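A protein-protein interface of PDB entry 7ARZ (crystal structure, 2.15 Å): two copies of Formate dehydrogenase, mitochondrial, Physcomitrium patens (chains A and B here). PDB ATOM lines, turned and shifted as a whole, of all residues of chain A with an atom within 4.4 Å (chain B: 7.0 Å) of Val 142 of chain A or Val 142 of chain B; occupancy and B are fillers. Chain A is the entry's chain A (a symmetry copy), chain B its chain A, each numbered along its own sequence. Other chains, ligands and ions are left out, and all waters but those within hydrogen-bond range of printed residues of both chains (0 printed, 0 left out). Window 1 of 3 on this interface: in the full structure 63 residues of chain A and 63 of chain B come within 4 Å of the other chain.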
ATOM      1  N   LEU A 138      25.494  23.635  -5.531  1.00  0.00           N
ATOM      2  CA  LEU A 138      25.801  25.086  -5.558  1.00  0.00           C
ATOM      3  C   LEU A 138      24.749  25.823  -4.714  1.00  0.00           C
ATOM      4  O   LEU A 138      25.140  26.566  -3.776  1.00  0.00           O
ATOM      5  CB  LEU A 138      25.827  25.581  -7.013  1.00  0.00           C
ATOM      6  CG  LEU A 138      26.243  27.043  -7.222  1.00  0.00           C
ATOM      7  CD1 LEU A 138      26.670  27.285  -8.662  1.00  0.00           C
ATOM      8  CD2 LEU A 138      25.142  28.016  -6.854  1.00  0.00           C
ATOM      9  N   ARG A 139      23.466  25.659  -5.047  1.00  0.00           N
ATOM     10  CA  ARG A 139      22.369  26.462  -4.439  1.00  0.00           C
ATOM     11  C   ARG A 139      22.242  26.133  -2.944  1.00  0.00           C
ATOM     12  O   ARG A 139      21.991  27.062  -2.182  1.00  0.00           O
ATOM     13  CB  ARG A 139      21.017  26.205  -5.104  1.00  0.00           C
ATOM     14  CG  ARG A 139      20.964  26.475  -6.598  1.00  0.00           C
ATOM     15  CD  ARG A 139      20.837  27.922  -7.013  1.00  0.00           C
ATOM     16  NE  ARG A 139      21.171  27.971  -8.429  1.00  0.00           N
ATOM     17  CZ  ARG A 139      20.710  28.824  -9.318  1.00  0.00           C
ATOM     18  NH1 ARG A 139      19.869  29.784  -8.974  1.00  0.00           N
ATOM     19  NH2 ARG A 139      21.119  28.707 -10.575  1.00  0.00           N
ATOM     20  N   ILE A 140      22.444  24.874  -2.558  1.00  0.00           N
ATOM     21  CA  ILE A 140      22.373  24.391  -1.137  1.00  0.00           C
ATOM     22  C   ILE A 140      23.435  25.137  -0.310  1.00  0.00           C
ATOM     23  O   ILE A 140      23.074  25.833   0.676  1.00  0.00           O
ATOM     24  CB  ILE A 140      22.534  22.854  -1.056  1.00  0.00           C
ATOM     25  CG1 ILE A 140      21.374  22.132  -1.746  1.00  0.00           C
ATOM     26  CG2 ILE A 140      22.709  22.385   0.393  1.00  0.00           C
ATOM     27  CD1 ILE A 140      21.520  20.628  -1.738  1.00  0.00           C
ATOM     28  N   LEU A 141      24.675  25.084  -0.785  1.00  0.00           N
ATOM     29  CA  LEU A 141      25.853  25.656  -0.102  1.00  0.00           C
ATOM     30  C   LEU A 141      25.724  27.171  -0.070  1.00  0.00           C
ATOM     31  O   LEU A 141      26.006  27.757   0.975  1.00  0.00           O
ATOM     32  CB  LEU A 141      27.120  25.207  -0.828  1.00  0.00           C
ATOM     33  CG  LEU A 141      27.431  23.731  -0.671  1.00  0.00           C
ATOM     34  CD1 LEU A 141      28.721  23.358  -1.378  1.00  0.00           C
ATOM     35  CD2 LEU A 141      27.537  23.370   0.795  1.00  0.00           C
ATOM     36  N   VAL A 142      25.351  27.780  -1.179  1.00  0.00           N
ATOM     37  CA  VAL A 142      25.127  29.248  -1.254  1.00  0.00           C
ATOM     38  C   VAL A 142      24.079  29.669  -0.209  1.00  0.00           C
ATOM     39  O   VAL A 142      24.218  30.760   0.376  1.00  0.00           O
ATOM     40  CB  VAL A 142      24.739  29.664  -2.687  1.00  0.00           C
ATOM     41  CG1 VAL A 142      24.133  31.058  -2.748  1.00  0.00           C
ATOM     42  CG2 VAL A 142      25.942  29.565  -3.630  1.00  0.00           C
ATOM     43  N   LEU A 143      23.028  28.887   0.007  1.00  0.00           N
ATOM     44  CA  LEU A 143      21.940  29.345   0.915  1.00  0.00           C
ATOM     45  C   LEU A 143      22.349  29.061   2.362  1.00  0.00           C
ATOM     46  O   LEU A 143      22.203  29.960   3.194  1.00  0.00           O
ATOM     47  CB  LEU A 143      20.636  28.633   0.580  1.00  0.00           C
ATOM     48  CG  LEU A 143      19.945  29.108  -0.689  1.00  0.00           C
ATOM     49  CD1 LEU A 143      18.814  28.159  -1.011  1.00  0.00           C
ATOM     50  CD2 LEU A 143      19.430  30.532  -0.556  1.00  0.00           C
ATOM     51  N   VAL A 144      22.867  27.857   2.616  1.00  0.00           N
ATOM     52  CA  VAL A 144      23.275  27.403   3.966  1.00  0.00           C
ATOM     53  C   VAL A 144      24.406  28.304   4.471  1.00  0.00           C
ATOM     54  O   VAL A 144      24.302  28.801   5.614  1.00  0.00           O
ATOM     55  CB  VAL A 144      23.648  25.916   3.977  1.00  0.00           C
ATOM     56  CG1 VAL A 144      24.378  25.522   5.249  1.00  0.00           C
ATOM     57  CG2 VAL A 144      22.427  25.048   3.750  1.00  0.00           C
ATOM     58  N   ARG A 145      25.397  28.571   3.626  1.00  0.00           N
ATOM     59  CA  ARG A 145      26.625  29.319   3.994  1.00  0.00           C
ATOM     60  C   ARG A 145      26.453  30.823   3.747  1.00  0.00           C
ATOM     61  O   ARG A 145      27.403  31.593   3.988  1.00  0.00           O
ATOM     62  CB  ARG A 145      27.782  28.673   3.231  1.00  0.00           C
ATOM     63  CG  ARG A 145      27.870  27.163   3.449  1.00  0.00           C
ATOM     64  CD  ARG A 145      29.179  26.568   2.949  1.00  0.00           C
ATOM     65  NE  ARG A 145      30.185  27.419   3.526  1.00  0.00           N
ATOM     66  CZ  ARG A 145      30.737  27.229   4.717  1.00  0.00           C
ATOM     67  NH1 ARG A 145      30.451  26.149   5.438  1.00  0.00           N
ATOM     68  NH2 ARG A 145      31.577  28.131   5.163  1.00  0.00           N
ATOM     69  N   ASN A 146      25.286  31.243   3.285  1.00  0.00           N
ATOM     70  CA  ASN A 146      24.948  32.667   3.062  1.00  0.00           C
ATOM     71  C   ASN A 146      25.966  33.390   2.178  1.00  0.00           C
ATOM     72  O   ASN A 146      26.268  34.576   2.455  1.00  0.00           O
ATOM     73  CB  ASN A 146      24.808  33.401   4.391  1.00  0.00           C
ATOM     74  CG  ASN A 146      23.824  34.543   4.286  1.00  0.00           C
ATOM     75  OD1 ASN A 146      22.947  34.533   3.434  1.00  0.00           O
ATOM     76  ND2 ASN A 146      23.986  35.547   5.118  1.00  0.00           N
ATOM     77  N   PHE A 147      26.372  32.800   1.055  1.00  0.00           N
ATOM     78  CA  PHE A 147      27.316  33.440   0.101  1.00  0.00           C
ATOM     79  C   PHE A 147      26.803  34.779  -0.454  1.00  0.00           C
ATOM     80  O   PHE A 147      27.580  35.753  -0.488  1.00  0.00           O
ATOM     81  CB  PHE A 147      27.623  32.510  -1.070  1.00  0.00           C
ATOM     82  CG  PHE A 147      28.396  33.160  -2.188  1.00  0.00           C
ATOM     83  CD1 PHE A 147      29.770  33.318  -2.104  1.00  0.00           C
ATOM     84  CD2 PHE A 147      27.750  33.605  -3.332  1.00  0.00           C
ATOM     85  CE1 PHE A 147      30.486  33.914  -3.135  1.00  0.00           C
ATOM     86  CE2 PHE A 147      28.460  34.203  -4.362  1.00  0.00           C
ATOM     87  CZ  PHE A 147      29.828  34.346  -4.265  1.00  0.00           C
ATOM     88  N   ALA A 311      18.421  32.572  -3.606  1.00  0.00           N
ATOM     89  CA  ALA A 311      19.539  32.222  -4.505  1.00  0.00           C
ATOM     90  C   ALA A 311      18.961  31.975  -5.906  1.00  0.00           C
ATOM     91  O   ALA A 311      19.231  30.887  -6.474  1.00  0.00           O
ATOM     92  CB  ALA A 311      20.285  31.039  -3.947  1.00  0.00           C
ATOM     93  N   GLU B 136      34.720  25.999  -0.275  1.00  0.00           N
ATOM     94  CA  GLU B 136      35.618  25.933  -1.445  1.00  0.00           C
ATOM     95  C   GLU B 136      34.856  25.304  -2.617  1.00  0.00           C
ATOM     96  O   GLU B 136      34.923  25.832  -3.736  1.00  0.00           O
ATOM     97  CB  GLU B 136      36.886  25.188  -1.056  1.00  0.00           C
ATOM     98  CG  GLU B 136      37.851  26.052  -0.276  1.00  0.00           C
ATOM     99  CD  GLU B 136      39.140  25.337   0.093  1.00  0.00           C
ATOM    100  OE1 GLU B 136      39.279  24.132  -0.223  1.00  0.00           O
ATOM    101  OE2 GLU B 136      39.989  25.987   0.718  1.00  0.00           O
ATOM    102  N   VAL B 137      34.109  24.237  -2.355  1.00  0.00           N
ATOM    103  CA  VAL B 137      33.213  23.621  -3.366  1.00  0.00           C
ATOM    104  C   VAL B 137      32.205  24.686  -3.809  1.00  0.00           C
ATOM    105  O   VAL B 137      32.046  24.895  -5.027  1.00  0.00           O
ATOM    106  CB  VAL B 137      32.535  22.358  -2.817  1.00  0.00           C
ATOM    107  CG1 VAL B 137      31.483  21.842  -3.775  1.00  0.00           C
ATOM    108  CG2 VAL B 137      33.542  21.265  -2.494  1.00  0.00           C
ATOM    109  N   LEU B 138      31.568  25.360  -2.854  1.00  0.00           N
ATOM    110  CA  LEU B 138      30.663  26.500  -3.139  1.00  0.00           C
ATOM    111  C   LEU B 138      31.334  27.408  -4.180  1.00  0.00           C
ATOM    112  O   LEU B 138      30.710  27.676  -5.240  1.00  0.00           O
ATOM    113  CB  LEU B 138      30.349  27.248  -1.833  1.00  0.00           C
ATOM    114  CG  LEU B 138      29.331  28.391  -1.937  1.00  0.00           C
ATOM    115  CD1 LEU B 138      28.768  28.741  -0.569  1.00  0.00           C
ATOM    116  CD2 LEU B 138      29.921  29.634  -2.571  1.00  0.00           C
ATOM    117  N   ARG B 139      32.543  27.895  -3.887  1.00  0.00           N
ATOM    118  CA  ARG B 139      33.215  28.934  -4.716  1.00  0.00           C
ATOM    119  C   ARG B 139      33.549  28.366  -6.103  1.00  0.00           C
ATOM    120  O   ARG B 139      33.413  29.114  -7.066  1.00  0.00           O
ATOM    121  CB  ARG B 139      34.508  29.444  -4.081  1.00  0.00           C
ATOM    122  CG  ARG B 139      34.361  30.039  -2.690  1.00  0.00           C
ATOM    123  CD  ARG B 139      33.828  31.451  -2.619  1.00  0.00           C
ATOM    124  NE  ARG B 139      33.433  31.667  -1.235  1.00  0.00           N
ATOM    125  CZ  ARG B 139      33.432  32.811  -0.586  1.00  0.00           C
ATOM    126  NH1 ARG B 139      33.792  33.936  -1.180  1.00  0.00           N
ATOM    127  NH2 ARG B 139      33.049  32.815   0.685  1.00  0.00           N
ATOM    128  N   ILE B 140      33.932  27.092  -6.184  1.00  0.00           N
ATOM    129  CA  ILE B 140      34.279  26.382  -7.462  1.00  0.00           C
ATOM    130  C   ILE B 140      33.043  26.387  -8.380  1.00  0.00           C
ATOM    131  O   ILE B 140      33.118  26.930  -9.514  1.00  0.00           O
ATOM    132  CB  ILE B 140      34.803  24.952  -7.187  1.00  0.00           C
ATOM    133  CG1 ILE B 140      36.123  24.979  -6.414  1.00  0.00           C
ATOM    134  CG2 ILE B 140      34.923  24.140  -8.482  1.00  0.00           C
ATOM    135  CD1 ILE B 140      36.643  23.601  -6.075  1.00  0.00           C
ATOM    136  N   LEU B 141      31.925  25.912  -7.841  1.00  0.00           N
ATOM    137  CA  LEU B 141      30.653  25.747  -8.573  1.00  0.00           C
ATOM    138  C   LEU B 141      30.115  27.119  -8.952  1.00  0.00           C
ATOM    139  O   LEU B 141      29.662  27.273 -10.086  1.00  0.00           O
ATOM    140  CB  LEU B 141      29.669  24.970  -7.700  1.00  0.00           C
ATOM    141  CG  LEU B 141      30.036  23.512  -7.505  1.00  0.00           C
ATOM    142  CD1 LEU B 141      29.000  22.788  -6.665  1.00  0.00           C
ATOM    143  CD2 LEU B 141      30.173  22.822  -8.844  1.00  0.00           C
ATOM    144  N   VAL B 142      30.130  28.061  -8.029  1.00  0.00           N
ATOM    145  CA  VAL B 142      29.692  29.457  -8.298  1.00  0.00           C
ATOM    146  C   VAL B 142      30.507  30.042  -9.464  1.00  0.00           C
ATOM    147  O   VAL B 142      29.941  30.804 -10.271  1.00  0.00           O
ATOM    148  CB  VAL B 142      29.787  30.310  -7.017  1.00  0.00           C
ATOM    149  CG1 VAL B 142      29.726  31.803  -7.303  1.00  0.00           C
ATOM    150  CG2 VAL B 142      28.698  29.916  -6.015  1.00  0.00           C
ATOM    151  N   LEU B 143      31.803  29.766  -9.553  1.00  0.00           N
ATOM    152  CA  LEU B 143      32.631  30.432 -10.596  1.00  0.00           C
ATOM    153  C   LEU B 143      32.461  29.682 -11.918  1.00  0.00           C
ATOM    154  O   LEU B 143      32.247  30.343 -12.938  1.00  0.00           O
ATOM    155  CB  LEU B 143      34.096  30.450 -10.177  1.00  0.00           C
ATOM    156  CG  LEU B 143      34.447  31.450  -9.086  1.00  0.00           C
ATOM    157  CD1 LEU B 143      35.858  31.183  -8.618  1.00  0.00           C
ATOM    158  CD2 LEU B 143      34.300  32.886  -9.561  1.00  0.00           C
ATOM    159  N   VAL B 144      32.529  28.349 -11.868  1.00  0.00           N
ATOM    160  CA  VAL B 144      32.429  27.473 -13.059  1.00  0.00           C
ATOM    161  C   VAL B 144      31.047  27.657 -13.693  1.00  0.00           C
ATOM    162  O   VAL B 144      30.985  27.879 -14.923  1.00  0.00           O
ATOM    163  CB  VAL B 144      32.737  26.011 -12.715  1.00  0.00           C
ATOM    164  CG1 VAL B 144      32.317  25.065 -13.826  1.00  0.00           C
ATOM    165  CG2 VAL B 144      34.200  25.832 -12.362  1.00  0.00           C
ATOM    166  N   ARG B 145      29.995  27.651 -12.880  1.00  0.00           N
ATOM    167  CA  ARG B 145      28.586  27.690 -13.342  1.00  0.00           C
ATOM    168  C   ARG B 145      28.077  29.133 -13.449  1.00  0.00           C
ATOM    169  O   ARG B 145      26.902  29.340 -13.808  1.00  0.00           O
ATOM    170  CB  ARG B 145      27.784  26.797 -12.395  1.00  0.00           C
ATOM    171  CG  ARG B 145      28.370  25.391 -12.262  1.00  0.00           C
ATOM    172  CD  ARG B 145      27.423  24.418 -11.574  1.00  0.00           C
ATOM    173  NE  ARG B 145      26.180  24.597 -12.275  1.00  0.00           N
ATOM    174  CZ  ARG B 145      25.827  23.924 -13.362  1.00  0.00           C
ATOM    175  NH1 ARG B 145      26.589  22.942 -13.835  1.00  0.00           N
ATOM    176  NH2 ARG B 145      24.704  24.247 -13.955  1.00  0.00           N
ATOM    177  N   ASN B 146      28.922  30.108 -13.155  1.00  0.00           N
ATOM    178  CA  ASN B 146      28.599  31.548 -13.275  1.00  0.00           C
ATOM    179  C   ASN B 146      27.323  31.938 -12.525  1.00  0.00           C
ATOM    180  O   ASN B 146      26.553  32.780 -13.046  1.00  0.00           O
ATOM    181  CB  ASN B 146      28.476  31.951 -14.741  1.00  0.00           C
ATOM    182  CG  ASN B 146      28.862  33.398 -14.947  1.00  0.00           C
ATOM    183  OD1 ASN B 146      29.611  33.959 -14.162  1.00  0.00           O
ATOM    184  ND2 ASN B 146      28.325  34.016 -15.974  1.00  0.00           N
ATOM    185  N   PHE B 147      27.155  31.500 -11.279  1.00  0.00           N
ATOM    186  CA  PHE B 147      25.978  31.865 -10.445  1.00  0.00           C
ATOM    187  C   PHE B 147      25.832  33.381 -10.233  1.00  0.00           C
ATOM    188  O   PHE B 147      24.710  33.902 -10.379  1.00  0.00           O
ATOM    189  CB  PHE B 147      26.044  31.183  -9.081  1.00  0.00           C
ATOM    190  CG  PHE B 147      25.009  31.667  -8.099  1.00  0.00           C
ATOM    191  CD1 PHE B 147      23.709  31.192  -8.145  1.00  0.00           C
ATOM    192  CD2 PHE B 147      25.339  32.593  -7.120  1.00  0.00           C
ATOM    193  CE1 PHE B 147      22.752  31.635  -7.239  1.00  0.00           C
ATOM    194  CE2 PHE B 147      24.387  33.039  -6.215  1.00  0.00           C
ATOM    195  CZ  PHE B 147      23.099  32.550  -6.271  1.00  0.00           C
ATOM    196  N   ALA B 148      26.886  34.082  -9.823  1.00  0.00           N
ATOM    197  CA  ALA B 148      26.757  35.425  -9.196  1.00  0.00           C
ATOM    198  C   ALA B 148      26.130  36.448 -10.153  1.00  0.00           C
ATOM    199  O   ALA B 148      25.220  37.167  -9.746  1.00  0.00           O
ATOM    200  CB  ALA B 148      28.077  35.910  -8.627  1.00  0.00           C
ATOM    201  N   PRO B 149      26.615  36.631 -11.405  1.00  0.00           N
ATOM    202  CA  PRO B 149      25.980  37.579 -12.326  1.00  0.00           C
ATOM    203  C   PRO B 149      24.480  37.313 -12.543  1.00  0.00           C
ATOM    204  O   PRO B 149      23.727  38.233 -12.665  1.00  0.00           O
ATOM    205  CB  PRO B 149      26.730  37.367 -13.649  1.00  0.00           C
ATOM    206  CG  PRO B 149      28.046  36.737 -13.267  1.00  0.00           C
ATOM    207  CD  PRO B 149      27.797  35.975 -11.980  1.00  0.00           C
ATOM    208  N   TRP B 151      22.418  35.812 -10.266  1.00  0.00           N
ATOM    209  CA  TRP B 151      21.713  36.230  -9.029  1.00  0.00           C
ATOM    210  C   TRP B 151      21.560  37.761  -9.054  1.00  0.00           C
ATOM    211  O   TRP B 151      20.421  38.271  -8.817  1.00  0.00           O
ATOM    212  CB  TRP B 151      22.455  35.718  -7.796  1.00  0.00           C
ATOM    213  CG  TRP B 151      21.844  36.189  -6.513  1.00  0.00           C
ATOM    214  CD1 TRP B 151      20.726  35.701  -5.911  1.00  0.00           C
ATOM    215  CD2 TRP B 151      22.304  37.270  -5.686  1.00  0.00           C
ATOM    216  NE1 TRP B 151      20.459  36.401  -4.762  1.00  0.00           N
ATOM    217  CE2 TRP B 151      21.409  37.368  -4.597  1.00  0.00           C
ATOM    218  CE3 TRP B 151      23.385  38.158  -5.750  1.00  0.00           C
ATOM    219  CZ2 TRP B 151      21.572  38.301  -3.577  1.00  0.00           C
ATOM    220  CZ3 TRP B 151      23.557  39.069  -4.732  1.00  0.00           C
ATOM    221  CH2 TRP B 151      22.665  39.130  -3.661  1.00  0.00           C
ATOM    222  N   HIS B 167      29.399  32.228 -20.260  1.00  0.00           N
ATOM    223  CA  HIS B 167      30.593  31.991 -19.399  1.00  0.00           C
ATOM    224  C   HIS B 167      30.227  31.010 -18.296  1.00  0.00           C
ATOM    225  O   HIS B 167      30.704  31.193 -17.186  1.00  0.00           O
ATOM    226  CB  HIS B 167      31.153  33.313 -18.834  1.00  0.00           C
ATOM    227  CG  HIS B 167      32.505  33.190 -18.210  1.00  0.00           C
ATOM    228  ND1 HIS B 167      33.561  32.580 -18.842  1.00  0.00           N
ATOM    229  CD2 HIS B 167      32.986  33.645 -17.035  1.00  0.00           C
ATOM    230  CE1 HIS B 167      34.634  32.633 -18.071  1.00  0.00           C
ATOM    231  NE2 HIS B 167      34.308  33.303 -16.963  1.00  0.00           N
ATOM    232  N   TYR B 261      40.093  28.497 -13.189  1.00  0.00           N
ATOM    233  CA  TYR B 261      39.490  29.147 -11.991  1.00  0.00           C
ATOM    234  C   TYR B 261      40.455  29.042 -10.799  1.00  0.00           C
ATOM    235  O   TYR B 261      41.105  28.017 -10.631  1.00  0.00           O
ATOM    236  CB  TYR B 261      38.090  28.570 -11.768  1.00  0.00           C
ATOM    237  CG  TYR B 261      37.165  28.721 -12.954  1.00  0.00           C
ATOM    238  CD1 TYR B 261      36.469  29.895 -13.166  1.00  0.00           C
ATOM    239  CD2 TYR B 261      37.006  27.706 -13.893  1.00  0.00           C
ATOM    240  CE1 TYR B 261      35.616  30.049 -14.251  1.00  0.00           C
ATOM    241  CE2 TYR B 261      36.164  27.849 -14.990  1.00  0.00           C
ATOM    242  CZ  TYR B 261      35.462  29.026 -15.169  1.00  0.00           C
ATOM    243  OH  TYR B 261      34.621  29.200 -16.238  1.00  0.00           O
ATOM    244  N   HIS B 310      34.387  37.616 -10.207  1.00  0.00           N
ATOM    245  CA  HIS B 310      34.893  37.315  -8.837  1.00  0.00           C
ATOM    246  C   HIS B 310      33.778  36.697  -7.993  1.00  0.00           C
ATOM    247  O   HIS B 310      32.585  37.009  -8.207  1.00  0.00           O
ATOM    248  CB  HIS B 310      35.564  38.519  -8.174  1.00  0.00           C
ATOM    249  CG  HIS B 310      34.636  39.432  -7.456  1.00  0.00           C
ATOM    250  ND1 HIS B 310      33.865  39.013  -6.391  1.00  0.00           N
ATOM    251  CD2 HIS B 310      34.403  40.753  -7.606  1.00  0.00           C
ATOM    252  CE1 HIS B 310      33.165  40.036  -5.938  1.00  0.00           C
ATOM    253  NE2 HIS B 310      33.479  41.117  -6.662  1.00  0.00           N
ATOM    254  N   ALA B 311      34.168  35.789  -7.106  1.00  0.00           N
ATOM    255  CA  ALA B 311      33.266  35.202  -6.094  1.00  0.00           C
ATOM    256  C   ALA B 311      33.820  35.552  -4.705  1.00  0.00           C
ATOM    257  O   ALA B 311      34.018  34.613  -3.894  1.00  0.00           O
ATOM    258  CB  ALA B 311      33.135  33.722  -6.332  1.00  0.00           C
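NH1 of Arg 139 of chain B lies within hydrogen-bond range of O of Ala 311 of chain B, at 2.8 Å.
The backbone carbonyl oxygen (O) of Val 142 of chain B sits at hydrogen-bond distance from the backbone NH (N) of Phe 147 of chain B, at 3.0 Å.
NH1 of Arg 139 of chain A is in hydrogen-bond range of O of Ala 311 of chain A, at 2.8 Å.
The backbone carbonyl oxygen of Val 142 of chain A is in hydrogen-bond range of the backbone NH of Phe 147 of chain A (3.0 Å).
Among the printed residues, merely in contact across the chains: Leu 138 of chain A with Leu 141 of chain B (3.3 Å), Leu 138 of chain A with Val 142 of chain B (3.6 Å), Leu 138 of chain A with Arg 145 of chain B (3.9 Å), Leu 138 of chain A with Phe 147 of chain B (3.7 Å), Arg 139 of chain A with Phe 147 of chain B (3.8 Å), Leu 141 of chain A with Val 137 of chain B (3.96 Å), Leu 141 of chain A with Leu 138 of chain B (3.3 Å), Val 142 of chain A with Leu 138 of chain B (3.6 Å), Val 142 of chain A with Val 142 of chain B (3.7 Å), Val 142 of chain A with Phe 147 of chain B (3.96 Å), Arg 145 of chain A with Leu 138 of chain B (3.9 Å), Phe 147 of chain A with Leu 138 of chain B (3.7 Å), Phe 147 of chain A with Arg 139 of chain B (3.8 Å), Phe 147 of chain A with Val 142 of chain B (3.96 Å), Phe 147 of chain A with Ala 311 of chain B (3.7 Å), Ala 311 of chain A with Phe 147 of chain B (3.7 Å) and Ala 311 of chain A with Trp 151 of chain B (3.9 Å).
Val 142 of chain A touches three residues of chain B.
Val 142 of chain B touches three residues of chain A.
Printed residues of chain A within 4 Å of Trp 151 of chain B: Ala 311.
Of the printed residues of chain B, Ala 311 of chain A touches Phe 147 and Trp 151.
Ile 140 of chain B touches none of the printed residues of chain A.
Val 144 of chain A touches none of the printed residues of chain B.
The nearest printed residue of chain B that does not touch Phe 147 of chain A is Phe 147 of chain B (4.5 Å).
Of the 19 printed residues of chain B, 9 touch a printed residue of chain A.
Of the 11 printed residues of chain A, 7 touch a printed residue of chain B.
Hydrophobic or aromatic side chains of chain A that line the printed part of chain B: Leu 138, Leu 141, Val 142, Phe 147 and Ala 311.
Among the printed residues, no Asp or Glu carboxylate lies within 4 Å of a Lys or Arg side-chain nitrogen of the other chain.
Leu 138 of chain A touches Val 142 of chain B, and with the chains exchanged Val 142 of chain A touches Leu 138 of chain B.
Leu 138 of chain A touches Arg 145 of chain B, and with the chains exchanged Arg 145 of chain A touches Leu 138 of chain B.
Leu 138 of chain A touches Phe 147 of chain B, and with the chains exchanged Phe 147 of chain A touches Leu 138 of chain B.
Arg 139 of chain A touches Phe 147 of chain B, and with the chains exchanged Phe 147 of chain A touches Arg 139 of chain B.
Of the 17 pairs that touch across the chains among the printed residues, 15 have their exchanged pair printed and touching as well.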
